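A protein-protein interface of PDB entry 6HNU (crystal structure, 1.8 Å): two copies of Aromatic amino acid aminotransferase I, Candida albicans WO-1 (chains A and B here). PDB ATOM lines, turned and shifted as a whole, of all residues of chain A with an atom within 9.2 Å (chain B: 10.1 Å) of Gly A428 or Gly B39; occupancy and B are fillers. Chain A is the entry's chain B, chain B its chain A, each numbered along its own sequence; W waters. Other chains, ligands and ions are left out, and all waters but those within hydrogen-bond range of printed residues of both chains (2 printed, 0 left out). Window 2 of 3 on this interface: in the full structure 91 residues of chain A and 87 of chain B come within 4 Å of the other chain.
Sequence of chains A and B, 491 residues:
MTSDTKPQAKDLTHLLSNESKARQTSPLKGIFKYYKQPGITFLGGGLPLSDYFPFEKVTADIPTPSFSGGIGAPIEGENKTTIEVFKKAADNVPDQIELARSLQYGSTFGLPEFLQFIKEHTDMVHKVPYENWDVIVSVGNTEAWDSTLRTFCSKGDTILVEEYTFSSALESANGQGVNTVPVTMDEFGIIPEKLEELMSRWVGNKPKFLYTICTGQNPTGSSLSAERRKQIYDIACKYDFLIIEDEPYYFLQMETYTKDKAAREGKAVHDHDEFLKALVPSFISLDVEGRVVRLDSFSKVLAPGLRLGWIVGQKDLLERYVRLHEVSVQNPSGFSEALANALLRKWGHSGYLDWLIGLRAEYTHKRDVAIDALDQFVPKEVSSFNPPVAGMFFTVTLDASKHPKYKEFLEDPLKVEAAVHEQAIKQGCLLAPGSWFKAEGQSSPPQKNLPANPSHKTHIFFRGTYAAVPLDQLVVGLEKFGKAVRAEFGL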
ATOM      1  N   VAL A 420     -22.623 -20.260  -5.800  1.00  0.00           N
ATOM      2  CA  VAL A 420     -21.555 -19.442  -6.434  1.00  0.00           C
ATOM      3  C   VAL A 420     -22.104 -18.061  -6.773  1.00  0.00           C
ATOM      4  O   VAL A 420     -21.386 -17.096  -6.518  1.00  0.00           O
ATOM      5  CB  VAL A 420     -20.935 -20.155  -7.647  1.00  0.00           C
ATOM      6  CG1 VAL A 420     -20.055 -19.211  -8.462  1.00  0.00           C
ATOM      7  CG2 VAL A 420     -20.166 -21.378  -7.199  1.00  0.00           C
ATOM      8  N   HIS A 421     -23.323 -17.969  -7.315  1.00  0.00           N
ATOM      9  CA  HIS A 421     -23.999 -16.672  -7.629  1.00  0.00           C
ATOM     10  C   HIS A 421     -24.109 -15.815  -6.369  1.00  0.00           C
ATOM     11  O   HIS A 421     -23.682 -14.658  -6.420  1.00  0.00           O
ATOM     12  CB  HIS A 421     -25.381 -16.902  -8.253  1.00  0.00           C
ATOM     13  CG  HIS A 421     -26.088 -15.685  -8.751  1.00  0.00           C
ATOM     14  ND1 HIS A 421     -25.515 -14.829  -9.668  1.00  0.00           N
ATOM     15  CD2 HIS A 421     -27.360 -15.256  -8.563  1.00  0.00           C
ATOM     16  CE1 HIS A 421     -26.390 -13.884  -9.966  1.00  0.00           C
ATOM     17  NE2 HIS A 421     -27.528 -14.131  -9.318  1.00  0.00           N
ATOM     18  N   GLU A 422     -24.619 -16.372  -5.268  1.00  0.00           N
ATOM     19  CA  GLU A 422     -24.755 -15.629  -3.981  1.00  0.00           C
ATOM     20  C   GLU A 422     -23.370 -15.165  -3.495  1.00  0.00           C
ATOM     21  O   GLU A 422     -23.225 -13.986  -3.091  1.00  0.00           O
ATOM     22  CB  GLU A 422     -25.472 -16.510  -2.944  1.00  0.00           C
ATOM     23  CG  GLU A 422     -26.926 -16.838  -3.296  1.00  0.00           C
ATOM     24  CD  GLU A 422     -27.548 -17.939  -2.440  1.00  0.00           C
ATOM     25  OE1 GLU A 422     -26.964 -18.217  -1.353  1.00  0.00           O
ATOM     26  OE2 GLU A 422     -28.611 -18.516  -2.847  1.00  0.00           O
ATOM     27  N   GLN A 423     -22.370 -16.047  -3.560  1.00  0.00           N
ATOM     28  CA  GLN A 423     -20.989 -15.744  -3.086  1.00  0.00           C
ATOM     29  C   GLN A 423     -20.376 -14.617  -3.944  1.00  0.00           C
ATOM     30  O   GLN A 423     -19.843 -13.668  -3.369  1.00  0.00           O
ATOM     31  CB  GLN A 423     -20.124 -17.006  -3.090  1.00  0.00           C
ATOM     32  CG  GLN A 423     -18.719 -16.755  -2.541  1.00  0.00           C
ATOM     33  CD  GLN A 423     -18.673 -16.588  -1.040  1.00  0.00           C
ATOM     34  OE1 GLN A 423     -18.088 -15.647  -0.520  1.00  0.00           O
ATOM     35  NE2 GLN A 423     -19.298 -17.511  -0.323  1.00  0.00           N
ATOM     36  N   ALA A 424     -20.459 -14.716  -5.270  1.00  0.00           N
ATOM     37  CA  ALA A 424     -20.043 -13.651  -6.219  1.00  0.00           C
ATOM     38  C   ALA A 424     -20.626 -12.316  -5.770  1.00  0.00           C
ATOM     39  O   ALA A 424     -19.849 -11.339  -5.651  1.00  0.00           O
ATOM     40  CB  ALA A 424     -20.499 -13.999  -7.627  1.00  0.00           C
ATOM     41  N   ILE A 425     -21.940 -12.260  -5.552  1.00  0.00           N
ATOM     42  CA  ILE A 425     -22.632 -11.001  -5.175  1.00  0.00           C
ATOM     43  C   ILE A 425     -22.046 -10.516  -3.841  1.00  0.00           C
ATOM     44  O   ILE A 425     -21.714  -9.330  -3.732  1.00  0.00           O
ATOM     45  CB  ILE A 425     -24.164 -11.175  -5.123  1.00  0.00           C
ATOM     46  CG1 ILE A 425     -24.763 -11.248  -6.529  1.00  0.00           C
ATOM     47  CG2 ILE A 425     -24.804 -10.049  -4.336  1.00  0.00           C
ATOM     48  CD1 ILE A 425     -26.006 -12.078  -6.620  1.00  0.00           C
ATOM     49  N   LYS A 426     -21.882 -11.416  -2.876  1.00  0.00           N
ATOM     50  CA  LYS A 426     -21.263 -11.062  -1.572  1.00  0.00           C
ATOM     51  C   LYS A 426     -19.826 -10.526  -1.803  1.00  0.00           C
ATOM     52  O   LYS A 426     -19.430  -9.618  -1.104  1.00  0.00           O
ATOM     53  CB  LYS A 426     -21.319 -12.274  -0.645  1.00  0.00           C
ATOM     54  CG  LYS A 426     -20.794 -12.034   0.766  1.00  0.00           C
ATOM     55  CD  LYS A 426     -20.602 -13.298   1.569  1.00  0.00           C
ATOM     56  CE  LYS A 426     -19.937 -13.054   2.912  1.00  0.00           C
ATOM     57  NZ  LYS A 426     -18.992 -14.145   3.229  1.00  0.00           N
ATOM     58  N   GLN A 427     -19.068 -11.063  -2.757  1.00  0.00           N
ATOM     59  CA  GLN A 427     -17.695 -10.585  -3.070  1.00  0.00           C
ATOM     60  C   GLN A 427     -17.729  -9.279  -3.881  1.00  0.00           C
ATOM     61  O   GLN A 427     -16.638  -8.730  -4.094  1.00  0.00           O
ATOM     62  CB  GLN A 427     -16.909 -11.652  -3.833  1.00  0.00           C
ATOM     63  CG  GLN A 427     -16.640 -12.938  -3.050  1.00  0.00           C
ATOM     64  CD  GLN A 427     -15.815 -12.758  -1.796  1.00  0.00           C
ATOM     65  OE1 GLN A 427     -14.925 -11.913  -1.725  1.00  0.00           O
ATOM     66  NE2 GLN A 427     -16.092 -13.590  -0.799  1.00  0.00           N
ATOM     67  N   GLY A 428     -18.904  -8.815  -4.336  1.00  0.00           N
ATOM     68  CA  GLY A 428     -19.079  -7.542  -5.074  1.00  0.00           C
ATOM     69  C   GLY A 428     -18.999  -7.677  -6.603  1.00  0.00           C
ATOM     70  O   GLY A 428     -18.558  -6.704  -7.269  1.00  0.00           O
ATOM     71  N   CYS A 429     -19.440  -8.792  -7.191  1.00  0.00           N
ATOM     72  CA  CYS A 429     -19.479  -8.957  -8.676  1.00  0.00           C
ATOM     73  C   CYS A 429     -20.700  -9.790  -9.061  1.00  0.00           C
ATOM     74  O   CYS A 429     -21.079 -10.721  -8.293  1.00  0.00           O
ATOM     75  CB  CYS A 429     -18.203  -9.662  -9.143  1.00  0.00           C
ATOM     76  SG  CYS A 429     -18.140 -10.204 -10.879  1.00  0.00           S
ATOM     77  N   LEU A 430     -21.287  -9.484 -10.213  1.00  0.00           N
ATOM     78  CA  LEU A 430     -22.467 -10.234 -10.687  1.00  0.00           C
ATOM     79  C   LEU A 430     -22.266 -10.712 -12.128  1.00  0.00           C
ATOM     80  O   LEU A 430     -21.936  -9.889 -13.024  1.00  0.00           O
ATOM     81  CB  LEU A 430     -23.692  -9.337 -10.536  1.00  0.00           C
ATOM     82  CG  LEU A 430     -24.993 -10.082 -10.790  1.00  0.00           C
ATOM     83  CD1 LEU A 430     -26.068  -9.660  -9.812  1.00  0.00           C
ATOM     84  CD2 LEU A 430     -25.434  -9.885 -12.237  1.00  0.00           C
ATOM     85  N   LEU A 431     -22.458 -12.017 -12.323  1.00  0.00           N
ATOM     86  CA  LEU A 431     -22.585 -12.672 -13.636  1.00  0.00           C
ATOM     87  C   LEU A 431     -23.966 -13.322 -13.717  1.00  0.00           C
ATOM     88  O   LEU A 431     -24.641 -13.469 -12.672  1.00  0.00           O
ATOM     89  CB  LEU A 431     -21.436 -13.676 -13.798  1.00  0.00           C
ATOM     90  CG  LEU A 431     -20.098 -13.070 -14.229  1.00  0.00           C
ATOM     91  CD1 LEU A 431     -19.418 -12.359 -13.088  1.00  0.00           C
ATOM     92  CD2 LEU A 431     -19.174 -14.119 -14.811  1.00  0.00           C
ATOM     93  N   GLN A 473     -12.621  -1.932 -14.220  1.00  0.00           N
ATOM     94  CA  GLN A 473     -13.738  -2.463 -13.389  1.00  0.00           C
ATOM     95  C   GLN A 473     -14.012  -3.915 -13.799  1.00  0.00           C
ATOM     96  O   GLN A 473     -14.384  -4.710 -12.906  1.00  0.00           O
ATOM     97  CB  GLN A 473     -14.974  -1.569 -13.473  1.00  0.00           C
ATOM     98  CG  GLN A 473     -14.761  -0.194 -12.858  1.00  0.00           C
ATOM     99  CD  GLN A 473     -13.962  -0.261 -11.575  1.00  0.00           C
ATOM    100  OE1 GLN A 473     -14.289  -1.015 -10.657  1.00  0.00           O
ATOM    101  NE2 GLN A 473     -12.898   0.528 -11.497  1.00  0.00           N
ATOM    102  N   LEU A 474     -13.784  -4.263 -15.068  1.00  0.00           N
ATOM    103  CA  LEU A 474     -13.852  -5.662 -15.546  1.00  0.00           C
ATOM    104  C   LEU A 474     -12.849  -6.510 -14.754  1.00  0.00           C
ATOM    105  O   LEU A 474     -13.238  -7.601 -14.260  1.00  0.00           O
ATOM    106  CB  LEU A 474     -13.551  -5.732 -17.043  1.00  0.00           C
ATOM    107  CG  LEU A 474     -13.464  -7.147 -17.605  1.00  0.00           C
ATOM    108  CD1 LEU A 474     -14.784  -7.876 -17.391  1.00  0.00           C
ATOM    109  CD2 LEU A 474     -13.112  -7.130 -19.080  1.00  0.00           C
ATOM    110  N   VAL A 476     -11.285  -5.925 -11.891  1.00  0.00           N
ATOM    111  CA  VAL A 476     -11.747  -5.890 -10.473  1.00  0.00           C
ATOM    112  C   VAL A 476     -12.819  -6.974 -10.309  1.00  0.00           C
ATOM    113  O   VAL A 476     -12.715  -7.803  -9.368  1.00  0.00           O
ATOM    114  CB  VAL A 476     -12.300  -4.504 -10.080  1.00  0.00           C
ATOM    115  CG1 VAL A 476     -13.111  -4.547  -8.788  1.00  0.00           C
ATOM    116  CG2 VAL A 476     -11.203  -3.450  -9.965  1.00  0.00           C
ATOM    117  N   GLY A 477     -13.833  -6.939 -11.182  1.00  0.00           N
ATOM    118  CA  GLY A 477     -14.995  -7.841 -11.109  1.00  0.00           C
ATOM    119  C   GLY A 477     -14.556  -9.280 -11.100  1.00  0.00           C
ATOM    120  O   GLY A 477     -15.003 -10.028 -10.215  1.00  0.00           O
ATOM    121  N   LEU A 478     -13.671  -9.638 -12.029  1.00  0.00           N
ATOM    122  CA  LEU A 478     -13.310 -11.042 -12.299  1.00  0.00           C
ATOM    123  C   LEU A 478     -12.346 -11.552 -11.227  1.00  0.00           C
ATOM    124  O   LEU A 478     -12.323 -12.775 -10.992  1.00  0.00           O
ATOM    125  CB  LEU A 478     -12.720 -11.083 -13.698  1.00  0.00           C
ATOM    126  CG  LEU A 478     -13.774 -10.958 -14.793  1.00  0.00           C
ATOM    127  CD1 LEU A 478     -13.126 -11.194 -16.134  1.00  0.00           C
ATOM    128  CD2 LEU A 478     -14.892 -11.964 -14.564  1.00  0.00           C
ATOM    129  N   GLU A 479     -11.612 -10.649 -10.583  1.00  0.00           N
ATOM    130  CA  GLU A 479     -10.793 -11.007  -9.393  1.00  0.00           C
ATOM    131  C   GLU A 479     -11.773 -11.388  -8.279  1.00  0.00           C
ATOM    132  O   GLU A 479     -11.605 -12.453  -7.706  1.00  0.00           O
ATOM    133  CB  GLU A 479      -9.848  -9.874  -8.986  1.00  0.00           C
ATOM    134  CG  GLU A 479      -9.184 -10.125  -7.638  1.00  0.00           C
ATOM    135  CD  GLU A 479      -7.903  -9.347  -7.394  1.00  0.00           C
ATOM    136  OE1 GLU A 479      -7.915  -8.113  -7.585  1.00  0.00           O
ATOM    137  OE2 GLU A 479      -6.898  -9.985  -7.007  1.00  0.00           O
ATOM    138  N   LYS A 480     -12.797 -10.571  -8.054  1.00  0.00           N
ATOM    139  CA  LYS A 480     -13.837 -10.850  -7.035  1.00  0.00           C
ATOM    140  C   LYS A 480     -14.536 -12.172  -7.374  1.00  0.00           C
ATOM    141  O   LYS A 480     -14.861 -12.902  -6.423  1.00  0.00           O
ATOM    142  CB  LYS A 480     -14.756  -9.641  -6.853  1.00  0.00           C
ATOM    143  CG  LYS A 480     -14.086  -8.445  -6.202  1.00  0.00           C
ATOM    144  CD  LYS A 480     -14.935  -7.193  -6.112  1.00  0.00           C
ATOM    145  CE  LYS A 480     -14.231  -6.104  -5.322  1.00  0.00           C
ATOM    146  NZ  LYS A 480     -14.865  -4.775  -5.507  1.00  0.00           N
ATOM    147  N   PHE A 481     -14.691 -12.528  -8.659  1.00  0.00           N
ATOM    148  CA  PHE A 481     -15.391 -13.767  -9.078  1.00  0.00           C
ATOM    149  C   PHE A 481     -14.491 -14.965  -8.778  1.00  0.00           C
ATOM    150  O   PHE A 481     -14.973 -16.001  -8.295  1.00  0.00           O
ATOM    151  CB  PHE A 481     -15.778 -13.749 -10.559  1.00  0.00           C
ATOM    152  CG  PHE A 481     -16.640 -14.913 -10.955  1.00  0.00           C
ATOM    153  CD1 PHE A 481     -17.969 -14.980 -10.571  1.00  0.00           C
ATOM    154  CD2 PHE A 481     -16.111 -15.985 -11.645  1.00  0.00           C
ATOM    155  CE1 PHE A 481     -18.756 -16.066 -10.920  1.00  0.00           C
ATOM    156  CE2 PHE A 481     -16.894 -17.079 -11.976  1.00  0.00           C
ATOM    157  CZ  PHE A 481     -18.213 -17.115 -11.612  1.00  0.00           C
ATOM    158  N   LYS A 483     -12.287 -15.113  -6.391  1.00  0.00           N
ATOM    159  CA  LYS A 483     -12.355 -15.253  -4.902  1.00  0.00           C
ATOM    160  C   LYS A 483     -13.606 -16.050  -4.519  1.00  0.00           C
ATOM    161  O   LYS A 483     -13.534 -16.906  -3.611  1.00  0.00           O
ATOM    162  CB  LYS A 483     -12.569 -13.924  -4.179  1.00  0.00           C
ATOM    163  CG  LYS A 483     -11.370 -13.019  -3.987  1.00  0.00           C
ATOM    164  CD  LYS A 483     -11.606 -12.048  -2.835  1.00  0.00           C
ATOM    165  CE  LYS A 483     -11.278 -10.611  -3.171  1.00  0.00           C
ATOM    166  NZ  LYS A 483      -9.812 -10.373  -3.217  1.00  0.00           N
ATOM    167  N   ALA A 484     -14.738 -15.712  -5.147  1.00  0.00           N
ATOM    168  CA  ALA A 484     -16.048 -16.318  -4.849  1.00  0.00           C
ATOM    169  C   ALA A 484     -15.973 -17.806  -5.187  1.00  0.00           C
ATOM    170  O   ALA A 484     -16.434 -18.642  -4.348  1.00  0.00           O
ATOM    171  CB  ALA A 484     -17.144 -15.573  -5.586  1.00  0.00           C
ATOM    172  N   TYR B  34     -29.445  -5.075  -8.826  1.00  0.00           N
ATOM    173  CA  TYR B  34     -27.988  -4.939  -8.552  1.00  0.00           C
ATOM    174  C   TYR B  34     -27.331  -3.989  -9.560  1.00  0.00           C
ATOM    175  O   TYR B  34     -26.157  -3.615  -9.337  1.00  0.00           O
ATOM    176  CB  TYR B  34     -27.276  -6.296  -8.627  1.00  0.00           C
ATOM    177  CG  TYR B  34     -27.756  -7.328  -7.639  1.00  0.00           C
ATOM    178  CD1 TYR B  34     -27.412  -7.260  -6.299  1.00  0.00           C
ATOM    179  CD2 TYR B  34     -28.532  -8.399  -8.050  1.00  0.00           C
ATOM    180  CE1 TYR B  34     -27.835  -8.223  -5.395  1.00  0.00           C
ATOM    181  CE2 TYR B  34     -28.963  -9.370  -7.163  1.00  0.00           C
ATOM    182  CZ  TYR B  34     -28.594  -9.293  -5.830  1.00  0.00           C
ATOM    183  OH  TYR B  34     -29.011 -10.258  -4.962  1.00  0.00           O
ATOM    184  N   TYR B  35     -28.049  -3.637 -10.636  1.00  0.00           N
ATOM    185  CA  TYR B  35     -27.501  -2.949 -11.836  1.00  0.00           C
ATOM    186  C   TYR B  35     -26.956  -1.565 -11.464  1.00  0.00           C
ATOM    187  O   TYR B  35     -25.872  -1.197 -11.970  1.00  0.00           O
ATOM    188  CB  TYR B  35     -28.555  -2.822 -12.936  1.00  0.00           C
ATOM    189  CG  TYR B  35     -28.049  -2.130 -14.174  1.00  0.00           C
ATOM    190  CD1 TYR B  35     -26.879  -2.544 -14.786  1.00  0.00           C
ATOM    191  CD2 TYR B  35     -28.726  -1.055 -14.727  1.00  0.00           C
ATOM    192  CE1 TYR B  35     -26.398  -1.917 -15.921  1.00  0.00           C
ATOM    193  CE2 TYR B  35     -28.260  -0.418 -15.867  1.00  0.00           C
ATOM    194  CZ  TYR B  35     -27.087  -0.848 -16.462  1.00  0.00           C
ATOM    195  OH  TYR B  35     -26.604  -0.235 -17.580  1.00  0.00           O
ATOM    196  N   LYS B  36     -27.685  -0.833 -10.621  1.00  0.00           N
ATOM    197  CA  LYS B  36     -27.287   0.511 -10.124  1.00  0.00           C
ATOM    198  C   LYS B  36     -26.210   0.400  -9.030  1.00  0.00           C
ATOM    199  O   LYS B  36     -25.309   1.253  -9.029  1.00  0.00           O
ATOM    200  CB  LYS B  36     -28.522   1.255  -9.601  1.00  0.00           C
ATOM    201  CG  LYS B  36     -29.118   0.721  -8.301  1.00  0.00           C
ATOM    202  CD  LYS B  36     -28.624   1.438  -7.047  1.00  0.00           C
ATOM    203  CE  LYS B  36     -29.079   0.770  -5.767  1.00  0.00           C
ATOM    204  NZ  LYS B  36     -30.443   1.191  -5.372  1.00  0.00           N
ATOM    205  N   GLN B  37     -26.304  -0.610  -8.151  1.00  0.00           N
ATOM    206  CA  GLN B  37     -25.743  -0.614  -6.767  1.00  0.00           C
ATOM    207  C   GLN B  37     -24.250  -0.296  -6.757  1.00  0.00           C
ATOM    208  O   GLN B  37     -23.466  -0.925  -7.468  1.00  0.00           O
ATOM    209  CB  GLN B  37     -25.988  -1.950  -6.061  1.00  0.00           C
ATOM    210  CG  GLN B  37     -27.330  -1.998  -5.346  1.00  0.00           C
ATOM    211  CD  GLN B  37     -27.368  -2.981  -4.205  1.00  0.00           C
ATOM    212  OE1 GLN B  37     -26.739  -4.037  -4.246  1.00  0.00           O
ATOM    213  NE2 GLN B  37     -28.117  -2.630  -3.172  1.00  0.00           N
ATOM    214  N   PRO B  38     -23.805   0.668  -5.912  1.00  0.00           N
ATOM    215  CA  PRO B  38     -22.382   0.848  -5.650  1.00  0.00           C
ATOM    216  C   PRO B  38     -21.874  -0.433  -4.974  1.00  0.00           C
ATOM    217  O   PRO B  38     -22.640  -1.086  -4.254  1.00  0.00           O
ATOM    218  CB  PRO B  38     -22.286   2.067  -4.717  1.00  0.00           C
ATOM    219  CG  PRO B  38     -23.668   2.716  -4.768  1.00  0.00           C
ATOM    220  CD  PRO B  38     -24.635   1.604  -5.134  1.00  0.00           C
ATOM    221  N   GLY B  39     -20.623  -0.791  -5.257  1.00  0.00           N
ATOM    222  CA  GLY B  39     -19.966  -1.974  -4.676  1.00  0.00           C
ATOM    223  C   GLY B  39     -20.164  -3.239  -5.500  1.00  0.00           C
ATOM    224  O   GLY B  39     -19.491  -4.206  -5.199  1.00  0.00           O
ATOM    225  N   ILE B  40     -21.073  -3.260  -6.481  1.00  0.00           N
ATOM    226  CA  ILE B  40     -21.270  -4.440  -7.373  1.00  0.00           C
ATOM    227  C   ILE B  40     -20.728  -4.105  -8.762  1.00  0.00           C
ATOM    228  O   ILE B  40     -21.250  -3.161  -9.385  1.00  0.00           O
ATOM    229  CB  ILE B  40     -22.749  -4.854  -7.483  1.00  0.00           C
ATOM    230  CG1 ILE B  40     -23.442  -4.983  -6.127  1.00  0.00           C
ATOM    231  CG2 ILE B  40     -22.860  -6.134  -8.291  1.00  0.00           C
ATOM    232  CD1 ILE B  40     -23.012  -6.184  -5.341  1.00  0.00           C
ATOM    233  N   THR B  41     -19.750  -4.865  -9.245  1.00  0.00           N
ATOM    234  CA  THR B  41     -19.344  -4.854 -10.673  1.00  0.00           C
ATOM    235  C   THR B  41     -20.319  -5.743 -11.437  1.00  0.00           C
ATOM    236  O   THR B  41     -20.290  -6.965 -11.221  1.00  0.00           O
ATOM    237  CB  THR B  41     -17.919  -5.339 -10.883  1.00  0.00           C
ATOM    238  OG1 THR B  41     -17.113  -4.606  -9.966  1.00  0.00           O
ATOM    239  CG2 THR B  41     -17.455  -5.112 -12.303  1.00  0.00           C
ATOM    240  N   PHE B  42     -21.197  -5.121 -12.220  1.00  0.00           N
ATOM    241  CA  PHE B  42     -22.352  -5.803 -12.850  1.00  0.00           C
ATOM    242  C   PHE B  42     -21.914  -6.266 -14.238  1.00  0.00           C
ATOM    243  O   PHE B  42     -21.836  -5.399 -15.129  1.00  0.00           O
ATOM    244  CB  PHE B  42     -23.570  -4.880 -12.833  1.00  0.00           C
ATOM    245  CG  PHE B  42     -24.824  -5.570 -13.301  1.00  0.00           C
ATOM    246  CD1 PHE B  42     -25.096  -5.682 -14.654  1.00  0.00           C
ATOM    247  CD2 PHE B  42     -25.716  -6.130 -12.397  1.00  0.00           C
ATOM    248  CE1 PHE B  42     -26.246  -6.316 -15.098  1.00  0.00           C
ATOM    249  CE2 PHE B  42     -26.869  -6.760 -12.848  1.00  0.00           C
ATOM    250  CZ  PHE B  42     -27.122  -6.857 -14.199  1.00  0.00           C
ATOM    251  N   LEU B  43     -21.598  -7.558 -14.395  1.00  0.00           N
ATOM    252  CA  LEU B  43     -21.198  -8.162 -15.686  1.00  0.00           C
ATOM    253  C   LEU B  43     -22.310  -9.090 -16.215  1.00  0.00           C
ATOM    254  O   LEU B  43     -22.020  -9.946 -17.080  1.00  0.00           O
ATOM    255  CB  LEU B  43     -19.892  -8.927 -15.509  1.00  0.00           C
ATOM    256  CG  LEU B  43     -18.725  -8.158 -14.862  1.00  0.00           C
ATOM    257  CD1 LEU B  43     -17.476  -9.033 -14.812  1.00  0.00           C
ATOM    258  CD2 LEU B  43     -18.429  -6.862 -15.607  1.00  0.00           C
ATOM    259  N   GLY B  44     -23.517  -8.988 -15.673  1.00  0.00           N
ATOM    260  CA  GLY B  44     -24.585  -9.985 -15.892  1.00  0.00           C
ATOM    261  C   GLY B  44     -25.527  -9.573 -17.018  1.00  0.00           C
ATOM    262  O   GLY B  44     -26.418 -10.358 -17.326  1.00  0.00           O
HETATM  263  O   HOH W   1     -17.010  -4.582  -7.349  1.00  0.00           O
HETATM  264  O   HOH W   2     -16.807  -2.062 -10.449  1.00  0.00           O
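Gly A428 touches just these residues of chain B: Gly B39 (3.4 Å), Ile B40 (3.5 Å) and Thr B41 (3.0 Å). Printed residues of chain B within 4 Å of Cys A429: Thr B41. Of the printed residues of chain B, Leu A474 touches Leu B43 (3.9 Å). Lys A480 touches none of the printed residues of chain B. Phe A481 touches none of the printed residues of chain B. No residue of chain A comes within 4 Å of Pro B38. Gly B39 touches just one residue of chain A: Gly A428 (3.4 Å). Printed residues of chain A within 4 Å of Gly B44: Leu A430 (3.2 Å). The nearest residue of chain B that does not touch Gly A428 is Phe B42 (5.8 Å). The nearest printed residue of chain B that does not touch Cys A429 is Leu B43 (4.2 Å).
No position is printed for both chains.
Printed residues of chain B that touch a printed residue of chain A: Tyr B34, Gly B39, Ile B40, Thr B41, Phe B42, Leu B43 and Gly B44. Hydrophobic or aromatic side chains of chain B within 4 Å of the printed part of chain A: Tyr B34, Ile B40, Phe B42 and Leu B43. Among the printed residues, no Asp or Glu carboxylate lies within 4 Å of a Lys or Arg side-chain nitrogen of the other chain.
Water W2 lies within hydrogen-bond range of OG1 of Thr B41 (2.6 Å) and OE1 of Gln A473 (2.7 Å). Water W1 lies within hydrogen-bond range of OG1 of Thr B41, O of Gly A428, NZ of Lys A480 and O of Gly B39.
O of Ala A424 is in hydrogen-bond range of N of Cys A429. O of Gly A477 is in hydrogen-bond range of SG of Cys A429.
The backbone NH (N) of Thr B41 sits at hydrogen-bond distance from the backbone carbonyl oxygen (O) of Gly A428. The backbone carbonyl oxygen (O) of Thr B41 lies within hydrogen-bond range of the backbone NH (N) of Leu A430 (2.9 Å). The backbone NH of Leu B43 lies within hydrogen-bond range of the backbone carbonyl oxygen of Leu A430 (2.7 Å). O of Leu A430 sits at hydrogen-bond distance from N of Gly B44, at 3.2 Å. O of Gly A428 sits close to O of Gly B39 (3.4 Å).
Ile A425 touches Tyr B34. O of Ile A425 touches CD1 of Ile B40, at 3.8 Å. Gly A428 touches Ile B40. CD1 of Leu A430 touches CD2 of Tyr B34, at 3.3 Å. Leu A430 touches Ile B40. Phe B42 touches Leu A430. O of Gln A473 touches CG2 of Thr B41 (3.2 Å). Leu A474 touches Leu B43 (CD1 to CD1, 3.9 Å). Thr B41 touches Gly A477. Leu B43 touches Leu A478 (CD1 to CD2, 3.9 Å).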
